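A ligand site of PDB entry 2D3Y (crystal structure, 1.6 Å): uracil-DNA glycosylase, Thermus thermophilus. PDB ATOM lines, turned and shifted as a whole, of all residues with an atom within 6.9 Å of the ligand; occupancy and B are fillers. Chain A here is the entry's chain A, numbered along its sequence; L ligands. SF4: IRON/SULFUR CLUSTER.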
ATOM      1  N   LEU A  10      -2.837   2.289  22.731  1.00  0.00           N
ATOM      2  CA  LEU A  10      -3.640   2.868  23.813  1.00  0.00           C
ATOM      3  C   LEU A  10      -3.237   2.245  25.148  1.00  0.00           C
ATOM      4  O   LEU A  10      -3.041   2.954  26.137  1.00  0.00           O
ATOM      5  CB  LEU A  10      -5.139   2.593  23.598  1.00  0.00           C
ATOM      6  CG  LEU A  10      -6.027   2.852  24.824  1.00  0.00           C
ATOM      7  CD1 LEU A  10      -6.014   4.323  25.189  1.00  0.00           C
ATOM      8  CD2 LEU A  10      -7.439   2.384  24.534  1.00  0.00           C
ATOM      9  N   THR A  11      -3.110   0.931  25.180  1.00  0.00           N
ATOM     10  CA  THR A  11      -2.770   0.259  26.432  1.00  0.00           C
ATOM     11  C   THR A  11      -1.377   0.578  26.957  1.00  0.00           C
ATOM     12  O   THR A  11      -1.063   0.254  28.103  1.00  0.00           O
ATOM     13  CB  THR A  11      -2.952  -1.264  26.323  1.00  0.00           C
ATOM     14  OG1 THR A  11      -2.107  -1.799  25.295  1.00  0.00           O
ATOM     15  CG2 THR A  11      -4.405  -1.593  25.987  1.00  0.00           C
ATOM     16  N   ALA A  12      -0.543   1.215  26.134  1.00  0.00           N
ATOM     17  CA  ALA A  12       0.808   1.590  26.537  1.00  0.00           C
ATOM     18  C   ALA A  12       0.856   3.045  27.018  1.00  0.00           C
ATOM     19  O   ALA A  12       1.878   3.503  27.542  1.00  0.00           O
ATOM     20  CB  ALA A  12       1.785   1.401  25.372  1.00  0.00           C
ATOM     21  N   CYS A  13      -0.246   3.768  26.842  1.00  0.00           N
ATOM     22  CA  CYS A  13      -0.303   5.176  27.211  1.00  0.00           C
ATOM     23  C   CYS A  13       0.007   5.463  28.682  1.00  0.00           C
ATOM     24  O   CYS A  13      -0.484   4.772  29.570  1.00  0.00           O
ATOM     25  CB  CYS A  13      -1.667   5.764  26.854  1.00  0.00           C
ATOM     26  SG  CYS A  13      -1.719   7.571  26.968  1.00  0.00           S
ATOM     27  N   ARG A  14       0.816   6.499  28.914  1.00  0.00           N
ATOM     28  CA  ARG A  14       1.217   6.913  30.251  1.00  0.00           C
ATOM     29  C   ARG A  14       1.242   8.446  30.345  1.00  0.00           C
ATOM     30  O   ARG A  14       2.078   9.020  31.046  1.00  0.00           O
ATOM     31  CB  ARG A  14       2.612   6.367  30.574  1.00  0.00           C
ATOM     32  CG  ARG A  14       2.720   4.839  30.586  1.00  0.00           C
ATOM     33  CD  ARG A  14       4.176   4.395  30.698  1.00  0.00           C
ATOM     34  NE  ARG A  14       4.800   4.821  31.947  1.00  0.00           N
ATOM     35  CZ  ARG A  14       4.618   4.214  33.114  1.00  0.00           C
ATOM     36  NH1 ARG A  14       3.851   3.140  33.199  1.00  0.00           N
ATOM     37  NH2 ARG A  14       5.210   4.686  34.206  1.00  0.00           N
ATOM     38  N   LEU A  15       0.320   9.094  29.647  1.00  0.00           N
ATOM     39  CA  LEU A  15       0.265  10.555  29.617  1.00  0.00           C
ATOM     40  C   LEU A  15      -0.147  11.262  30.900  1.00  0.00           C
ATOM     41  O   LEU A  15       0.377  12.326  31.219  1.00  0.00           O
ATOM     42  CB  LEU A  15      -0.669  11.010  28.494  1.00  0.00           C
ATOM     43  CG  LEU A  15      -0.243  10.719  27.056  1.00  0.00           C
ATOM     44  CD1 LEU A  15      -1.342  11.153  26.097  1.00  0.00           C
ATOM     45  CD2 LEU A  15       1.051  11.451  26.752  1.00  0.00           C
ATOM     46  N   CYS A  16      -1.088  10.685  31.635  1.00  0.00           N
ATOM     47  CA  CYS A  16      -1.600  11.304  32.862  1.00  0.00           C
ATOM     48  C   CYS A  16      -0.919  10.748  34.117  1.00  0.00           C
ATOM     49  O   CYS A  16      -1.227   9.651  34.576  1.00  0.00           O
ATOM     50  CB  CYS A  16      -3.110  11.112  32.925  1.00  0.00           C
ATOM     51  SG  CYS A  16      -3.977  11.663  31.412  1.00  0.00           S
ATOM     52  N   PRO A  17       0.005  11.525  34.712  1.00  0.00           N
ATOM     53  CA  PRO A  17       0.709  11.068  35.905  1.00  0.00           C
ATOM     54  C   PRO A  17      -0.159  10.559  37.059  1.00  0.00           C
ATOM     55  O   PRO A  17       0.143   9.521  37.658  1.00  0.00           O
ATOM     56  CB  PRO A  17       1.568  12.271  36.297  1.00  0.00           C
ATOM     57  CG  PRO A  17       0.774  13.435  35.792  1.00  0.00           C
ATOM     58  CD  PRO A  17       0.296  12.952  34.447  1.00  0.00           C
ATOM     59  N   LEU A  19      -3.172   9.332  36.938  1.00  0.00           N
ATOM     60  CA  LEU A  19      -3.871   8.111  36.556  1.00  0.00           C
ATOM     61  C   LEU A  19      -2.967   6.896  36.335  1.00  0.00           C
ATOM     62  O   LEU A  19      -3.379   5.761  36.583  1.00  0.00           O
ATOM     63  CB  LEU A  19      -4.726   8.385  35.323  1.00  0.00           C
ATOM     64  CG  LEU A  19      -5.631   9.618  35.469  1.00  0.00           C
ATOM     65  CD1 LEU A  19      -6.596   9.706  34.294  1.00  0.00           C
ATOM     66  CD2 LEU A  19      -6.401   9.538  36.791  1.00  0.00           C
ATOM     67  N   VAL A  20      -1.752   7.123  35.850  1.00  0.00           N
ATOM     68  CA  VAL A  20      -0.822   6.019  35.654  1.00  0.00           C
ATOM     69  C   VAL A  20      -0.521   5.452  37.027  1.00  0.00           C
ATOM     70  O   VAL A  20      -0.441   4.237  37.222  1.00  0.00           O
ATOM     71  CB  VAL A  20       0.488   6.502  34.995  1.00  0.00           C
ATOM     72  CG1 VAL A  20       1.543   5.389  35.044  1.00  0.00           C
ATOM     73  CG2 VAL A  20       0.220   6.905  33.544  1.00  0.00           C
ATOM     74  N   ARG A  23      -4.121   3.859  38.646  1.00  0.00           N
ATOM     75  CA  ARG A  23      -4.604   2.609  38.060  1.00  0.00           C
ATOM     76  C   ARG A  23      -3.848   1.407  38.609  1.00  0.00           C
ATOM     77  O   ARG A  23      -4.389   0.304  38.665  1.00  0.00           O
ATOM     78  CB  ARG A  23      -4.520   2.669  36.526  1.00  0.00           C
ATOM     79  CG  ARG A  23      -3.121   2.673  35.944  1.00  0.00           C
ATOM     80  CD  ARG A  23      -3.143   3.154  34.494  1.00  0.00           C
ATOM     81  NE  ARG A  23      -1.872   2.875  33.825  1.00  0.00           N
ATOM     82  CZ  ARG A  23      -1.449   3.484  32.709  1.00  0.00           C
ATOM     83  NH1 ARG A  23      -0.274   3.157  32.187  1.00  0.00           N
ATOM     84  NH2 ARG A  23      -2.188   4.429  32.139  1.00  0.00           N
ATOM     85  N   ARG A  41      -4.486  -0.804  33.457  1.00  0.00           N
ATOM     86  CA  ARG A  41      -3.984  -0.134  32.275  1.00  0.00           C
ATOM     87  C   ARG A  41      -5.157   0.568  31.583  1.00  0.00           C
ATOM     88  O   ARG A  41      -6.307   0.400  31.984  1.00  0.00           O
ATOM     89  CB  ARG A  41      -3.370  -1.149  31.305  1.00  0.00           C
ATOM     90  CG  ARG A  41      -2.099  -1.810  31.809  1.00  0.00           C
ATOM     91  CD  ARG A  41      -1.522  -2.756  30.770  1.00  0.00           C
ATOM     92  NE  ARG A  41      -2.259  -4.013  30.669  1.00  0.00           N
ATOM     93  CZ  ARG A  41      -2.186  -4.997  31.571  1.00  0.00           C
ATOM     94  NH1 ARG A  41      -2.899  -6.111  31.398  1.00  0.00           N
ATOM     95  NH2 ARG A  41      -1.407  -4.873  32.635  1.00  0.00           N
ATOM     96  N   PRO A  42      -4.872   1.374  30.542  1.00  0.00           N
ATOM     97  CA  PRO A  42      -5.964   2.067  29.846  1.00  0.00           C
ATOM     98  C   PRO A  42      -6.945   1.029  29.321  1.00  0.00           C
ATOM     99  O   PRO A  42      -6.550  -0.031  28.843  1.00  0.00           O
ATOM    100  CB  PRO A  42      -5.236   2.791  28.710  1.00  0.00           C
ATOM    101  CG  PRO A  42      -3.881   3.061  29.308  1.00  0.00           C
ATOM    102  CD  PRO A  42      -3.559   1.769  30.003  1.00  0.00           C
ATOM    103  N   VAL A  43      -8.236   1.343  29.407  1.00  0.00           N
ATOM    104  CA  VAL A  43      -9.283   0.406  28.986  1.00  0.00           C
ATOM    105  C   VAL A  43      -9.780   0.611  27.552  1.00  0.00           C
ATOM    106  O   VAL A  43     -10.333   1.659  27.224  1.00  0.00           O
ATOM    107  CB  VAL A  43     -10.500   0.512  29.938  1.00  0.00           C
ATOM    108  CG1 VAL A  43     -11.591  -0.469  29.515  1.00  0.00           C
ATOM    109  CG2 VAL A  43     -10.057   0.237  31.370  1.00  0.00           C
ATOM    110  N   ALA A 112     -14.884   8.728  27.989  1.00  0.00           N
ATOM    111  CA  ALA A 112     -14.073   9.917  27.721  1.00  0.00           C
ATOM    112  C   ALA A 112     -12.644   9.795  28.223  1.00  0.00           C
ATOM    113  O   ALA A 112     -11.709  10.297  27.591  1.00  0.00           O
ATOM    114  CB  ALA A 112     -14.737  11.143  28.322  1.00  0.00           C
ATOM    115  N   VAL A 113     -12.483   9.144  29.374  1.00  0.00           N
ATOM    116  CA  VAL A 113     -11.173   8.938  29.982  1.00  0.00           C
ATOM    117  C   VAL A 113     -11.026   7.423  30.088  1.00  0.00           C
ATOM    118  O   VAL A 113     -11.982   6.723  30.423  1.00  0.00           O
ATOM    119  CB  VAL A 113     -11.098   9.625  31.367  1.00  0.00           C
ATOM    120  CG1 VAL A 113      -9.937   9.085  32.176  1.00  0.00           C
ATOM    121  CG2 VAL A 113     -10.949  11.130  31.170  1.00  0.00           C
ATOM    122  N   ARG A 114      -9.844   6.914  29.801  1.00  0.00           N
ATOM    123  CA  ARG A 114      -9.648   5.474  29.781  1.00  0.00           C
ATOM    124  C   ARG A 114      -8.839   4.847  30.905  1.00  0.00           C
ATOM    125  O   ARG A 114      -8.555   3.638  30.879  1.00  0.00           O
ATOM    126  CB  ARG A 114      -9.111   5.099  28.396  1.00  0.00           C
ATOM    127  CG  ARG A 114     -10.090   5.519  27.295  1.00  0.00           C
ATOM    128  CD  ARG A 114      -9.496   5.586  25.899  1.00  0.00           C
ATOM    129  NE  ARG A 114     -10.549   5.858  24.915  1.00  0.00           N
ATOM    130  CZ  ARG A 114     -11.091   7.060  24.705  1.00  0.00           C
ATOM    131  NH1 ARG A 114     -10.682   8.116  25.385  1.00  0.00           N
ATOM    132  NH2 ARG A 114     -12.068   7.185  23.820  1.00  0.00           N
ATOM    133  N   CYS A 115      -8.493   5.647  31.904  1.00  0.00           N
ATOM    134  CA  CYS A 115      -7.770   5.160  33.075  1.00  0.00           C
ATOM    135  C   CYS A 115      -8.551   5.567  34.310  1.00  0.00           C
ATOM    136  O   CYS A 115      -9.073   6.678  34.382  1.00  0.00           O
ATOM    137  CB  CYS A 115      -6.355   5.738  33.129  1.00  0.00           C
ATOM    138  SG  CYS A 115      -5.273   5.091  31.845  1.00  0.00           S
ATOM    139  N   ALA A 116      -8.628   4.664  35.273  1.00  0.00           N
ATOM    140  CA  ALA A 116      -9.369   4.894  36.502  1.00  0.00           C
ATOM    141  C   ALA A 116      -8.871   6.103  37.302  1.00  0.00           C
ATOM    142  O   ALA A 116      -7.723   6.155  37.708  1.00  0.00           O
ATOM    143  CB  ALA A 116      -9.331   3.658  37.383  1.00  0.00           C
ATOM    144  N   GLU A 126      -6.842  15.820  32.315  1.00  0.00           N
ATOM    145  CA  GLU A 126      -6.870  14.408  31.950  1.00  0.00           C
ATOM    146  C   GLU A 126      -7.873  14.206  30.823  1.00  0.00           C
ATOM    147  O   GLU A 126      -7.613  13.461  29.867  1.00  0.00           O
ATOM    148  CB  GLU A 126      -7.219  13.562  33.186  1.00  0.00           C
ATOM    149  CG  GLU A 126      -6.110  13.586  34.238  1.00  0.00           C
ATOM    150  CD  GLU A 126      -6.536  13.148  35.632  1.00  0.00           C
ATOM    151  OE1 GLU A 126      -7.742  12.998  35.876  1.00  0.00           O
ATOM    152  OE2 GLU A 126      -5.638  12.978  36.492  1.00  0.00           O
ATOM    153  N   LEU A 127      -9.023  14.875  30.917  1.00  0.00           N
ATOM    154  CA  LEU A 127     -10.035  14.774  29.872  1.00  0.00           C
ATOM    155  C   LEU A 127      -9.493  15.287  28.538  1.00  0.00           C
ATOM    156  O   LEU A 127      -9.740  14.699  27.492  1.00  0.00           O
ATOM    157  CB  LEU A 127     -11.277  15.579  30.271  1.00  0.00           C
ATOM    158  CG  LEU A 127     -12.187  14.892  31.300  1.00  0.00           C
ATOM    159  CD1 LEU A 127     -13.006  15.933  32.035  1.00  0.00           C
ATOM    160  CD2 LEU A 127     -13.079  13.869  30.604  1.00  0.00           C
ATOM    161  N   ARG A 128      -8.747  16.390  28.580  1.00  0.00           N
ATOM    162  CA  ARG A 128      -8.192  16.948  27.357  1.00  0.00           C
ATOM    163  C   ARG A 128      -7.141  16.010  26.773  1.00  0.00           C
ATOM    164  O   ARG A 128      -7.011  15.900  25.550  1.00  0.00           O
ATOM    165  CB  ARG A 128      -7.564  18.329  27.624  1.00  0.00           C
ATOM    166  CG  ARG A 128      -8.595  19.418  27.939  1.00  0.00           C
ATOM    167  CD  ARG A 128      -7.992  20.803  27.750  1.00  0.00           C
ATOM    168  NE  ARG A 128      -6.926  21.082  28.718  1.00  0.00           N
ATOM    169  CZ  ARG A 128      -7.119  21.368  29.993  1.00  0.00           C
ATOM    170  NH1 ARG A 128      -8.354  21.430  30.488  1.00  0.00           N
ATOM    171  NH2 ARG A 128      -6.084  21.594  30.786  1.00  0.00           N
ATOM    172  N   ALA A 129      -6.424  15.319  27.640  1.00  0.00           N
ATOM    173  CA  ALA A 129      -5.399  14.387  27.194  1.00  0.00           C
ATOM    174  C   ALA A 129      -5.976  13.162  26.502  1.00  0.00           C
ATOM    175  O   ALA A 129      -5.547  12.794  25.409  1.00  0.00           O
ATOM    176  CB  ALA A 129      -4.527  13.955  28.374  1.00  0.00           C
ATOM    177  N   CYS A 130      -6.971  12.533  27.126  1.00  0.00           N
ATOM    178  CA  CYS A 130      -7.552  11.314  26.561  1.00  0.00           C
ATOM    179  C   CYS A 130      -8.380  11.556  25.310  1.00  0.00           C
ATOM    180  O   CYS A 130      -8.734  10.615  24.604  1.00  0.00           O
ATOM    181  CB  CYS A 130      -8.378  10.585  27.614  1.00  0.00           C
ATOM    182  SG  CYS A 130      -8.227   8.785  27.497  1.00  0.00           S
ATOM    183  N   ALA A 131      -8.688  12.826  25.025  1.00  0.00           N
ATOM    184  CA  ALA A 131      -9.465  13.152  23.840  1.00  0.00           C
ATOM    185  C   ALA A 131      -8.743  12.663  22.585  1.00  0.00           C
ATOM    186  O   ALA A 131      -9.364  12.429  21.552  1.00  0.00           O
ATOM    187  CB  ALA A 131      -9.698  14.662  23.756  1.00  0.00           C
ATOM    188  N   ARG A 132      -7.421  12.509  22.663  1.00  0.00           N
ATOM    189  CA  ARG A 132      -6.668  12.036  21.495  1.00  0.00           C
ATOM    190  C   ARG A 132      -7.065  10.594  21.174  1.00  0.00           C
ATOM    191  O   ARG A 132      -7.056  10.181  20.014  1.00  0.00           O
ATOM    192  CB  ARG A 132      -5.151  12.135  21.748  1.00  0.00           C
ATOM    193  CG  ARG A 132      -4.592  11.131  22.735  1.00  0.00           C
ATOM    194  CD  ARG A 132      -3.161  11.506  23.088  1.00  0.00           C
ATOM    195  NE  ARG A 132      -3.131  12.821  23.706  1.00  0.00           N
ATOM    196  CZ  ARG A 132      -2.042  13.564  23.854  1.00  0.00           C
ATOM    197  NH1 ARG A 132      -0.867  13.121  23.423  1.00  0.00           N
ATOM    198  NH2 ARG A 132      -2.122  14.756  24.427  1.00  0.00           N
ATOM    199  N   TRP A 133      -7.422   9.839  22.214  1.00  0.00           N
ATOM    200  CA  TRP A 133      -7.831   8.461  22.026  1.00  0.00           C
ATOM    201  C   TRP A 133      -9.290   8.388  21.578  1.00  0.00           C
ATOM    202  O   TRP A 133      -9.695   7.452  20.888  1.00  0.00           O
ATOM    203  CB  TRP A 133      -7.596   7.670  23.315  1.00  0.00           C
ATOM    204  CG  TRP A 133      -6.146   7.582  23.639  1.00  0.00           C
ATOM    205  CD1 TRP A 133      -5.530   8.029  24.773  1.00  0.00           C
ATOM    206  CD2 TRP A 133      -5.111   7.036  22.806  1.00  0.00           C
ATOM    207  NE1 TRP A 133      -4.173   7.803  24.701  1.00  0.00           N
ATOM    208  CE2 TRP A 133      -3.884   7.188  23.504  1.00  0.00           C
ATOM    209  CE3 TRP A 133      -5.101   6.434  21.545  1.00  0.00           C
ATOM    210  CZ2 TRP A 133      -2.666   6.760  22.976  1.00  0.00           C
ATOM    211  CZ3 TRP A 133      -3.875   6.003  21.023  1.00  0.00           C
ATOM    212  CH2 TRP A 133      -2.673   6.172  21.744  1.00  0.00           C
HETATM  213 FE1  SF4 L   1      -3.499   7.973  28.448  1.00  0.00          FE
HETATM  214 FE2  SF4 L   1      -4.960   6.981  30.489  1.00  0.00          FE
HETATM  215 FE3  SF4 L   1      -4.479   9.640  30.325  1.00  0.00          FE
HETATM  216 FE4  SF4 L   1      -6.151   8.447  28.576  1.00  0.00          FE
HETATM  217  S1  SF4 L   1      -6.446   8.647  30.802  1.00  0.00           S
HETATM  218  S2  SF4 L   1      -4.541   9.933  28.081  1.00  0.00           S
HETATM  219  S3  SF4 L   1      -5.159   6.445  28.307  1.00  0.00           S
HETATM  220  S4  SF4 L   1      -2.953   8.000  30.637  1.00  0.00           S
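O of Ala 112 sits at hydrogen-bond distance from NH1 of Arg 114 (3.3 Å). SG of Cys 115 lies close to NH2 of Arg 23, at 3.2 Å. The backbone carbonyl oxygen (O) of Cys 13 sits at hydrogen-bond distance from the guanidinium group (NH1) of Arg 23 (3.1 Å). The backbone carbonyl oxygen of Cys 130 lies within hydrogen-bond range of the guanidinium group of Arg 114 (3.3 Å). SG of Cys 13 sits close to N of Leu 15, at 3.7 Å. The indole nitrogen of Trp 133 lies close to the side-chain sulfur of Cys 13, at 3.3 Å. SG of Cys 130 lies close to O of Ala 112. NE of Arg 132 is in hydrogen-bond range of O of Ala 129 (3.0 Å).
FE1 of the ligand is bound by SG of Cys 13 (2.3 Å). SG of Cys 130 is bound to FE4 of the ligand, at 2.4 Å. A sulfur (S2) of the ligand lies close to the backbone NH of Cys 130 (3.7 Å). SG of Cys 16 binds FE3 of the ligand (2.4 Å). FE2 of the ligand is bound by SG of Cys 115 (2.3 Å). A sulfur (S4) of the ligand lies close to the backbone NH (N) of Leu 15 (3.6 Å). N of Cys 115 lies close to S1 of the ligand. N of Cys 16 sits close to S4 of the ligand.
Residues that only touch the ligand: Leu 10 (3.9 Å), Leu 19 (3.7 Å), Arg 23 (3.9 Å), Pro 42 (3.7 Å), Val 113 (3.8 Å), Arg 114 (3.9 Å), Ala 129 (3.9 Å) and Trp 133 (3.8 Å). Within 4 Å of the ligand: Leu 10, Cys 13, Leu 15, Cys 16, Leu 19, Arg 23, Pro 42, Val 113, Arg 114, Cys 115, Ala 129, Cys 130 and Trp 133.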
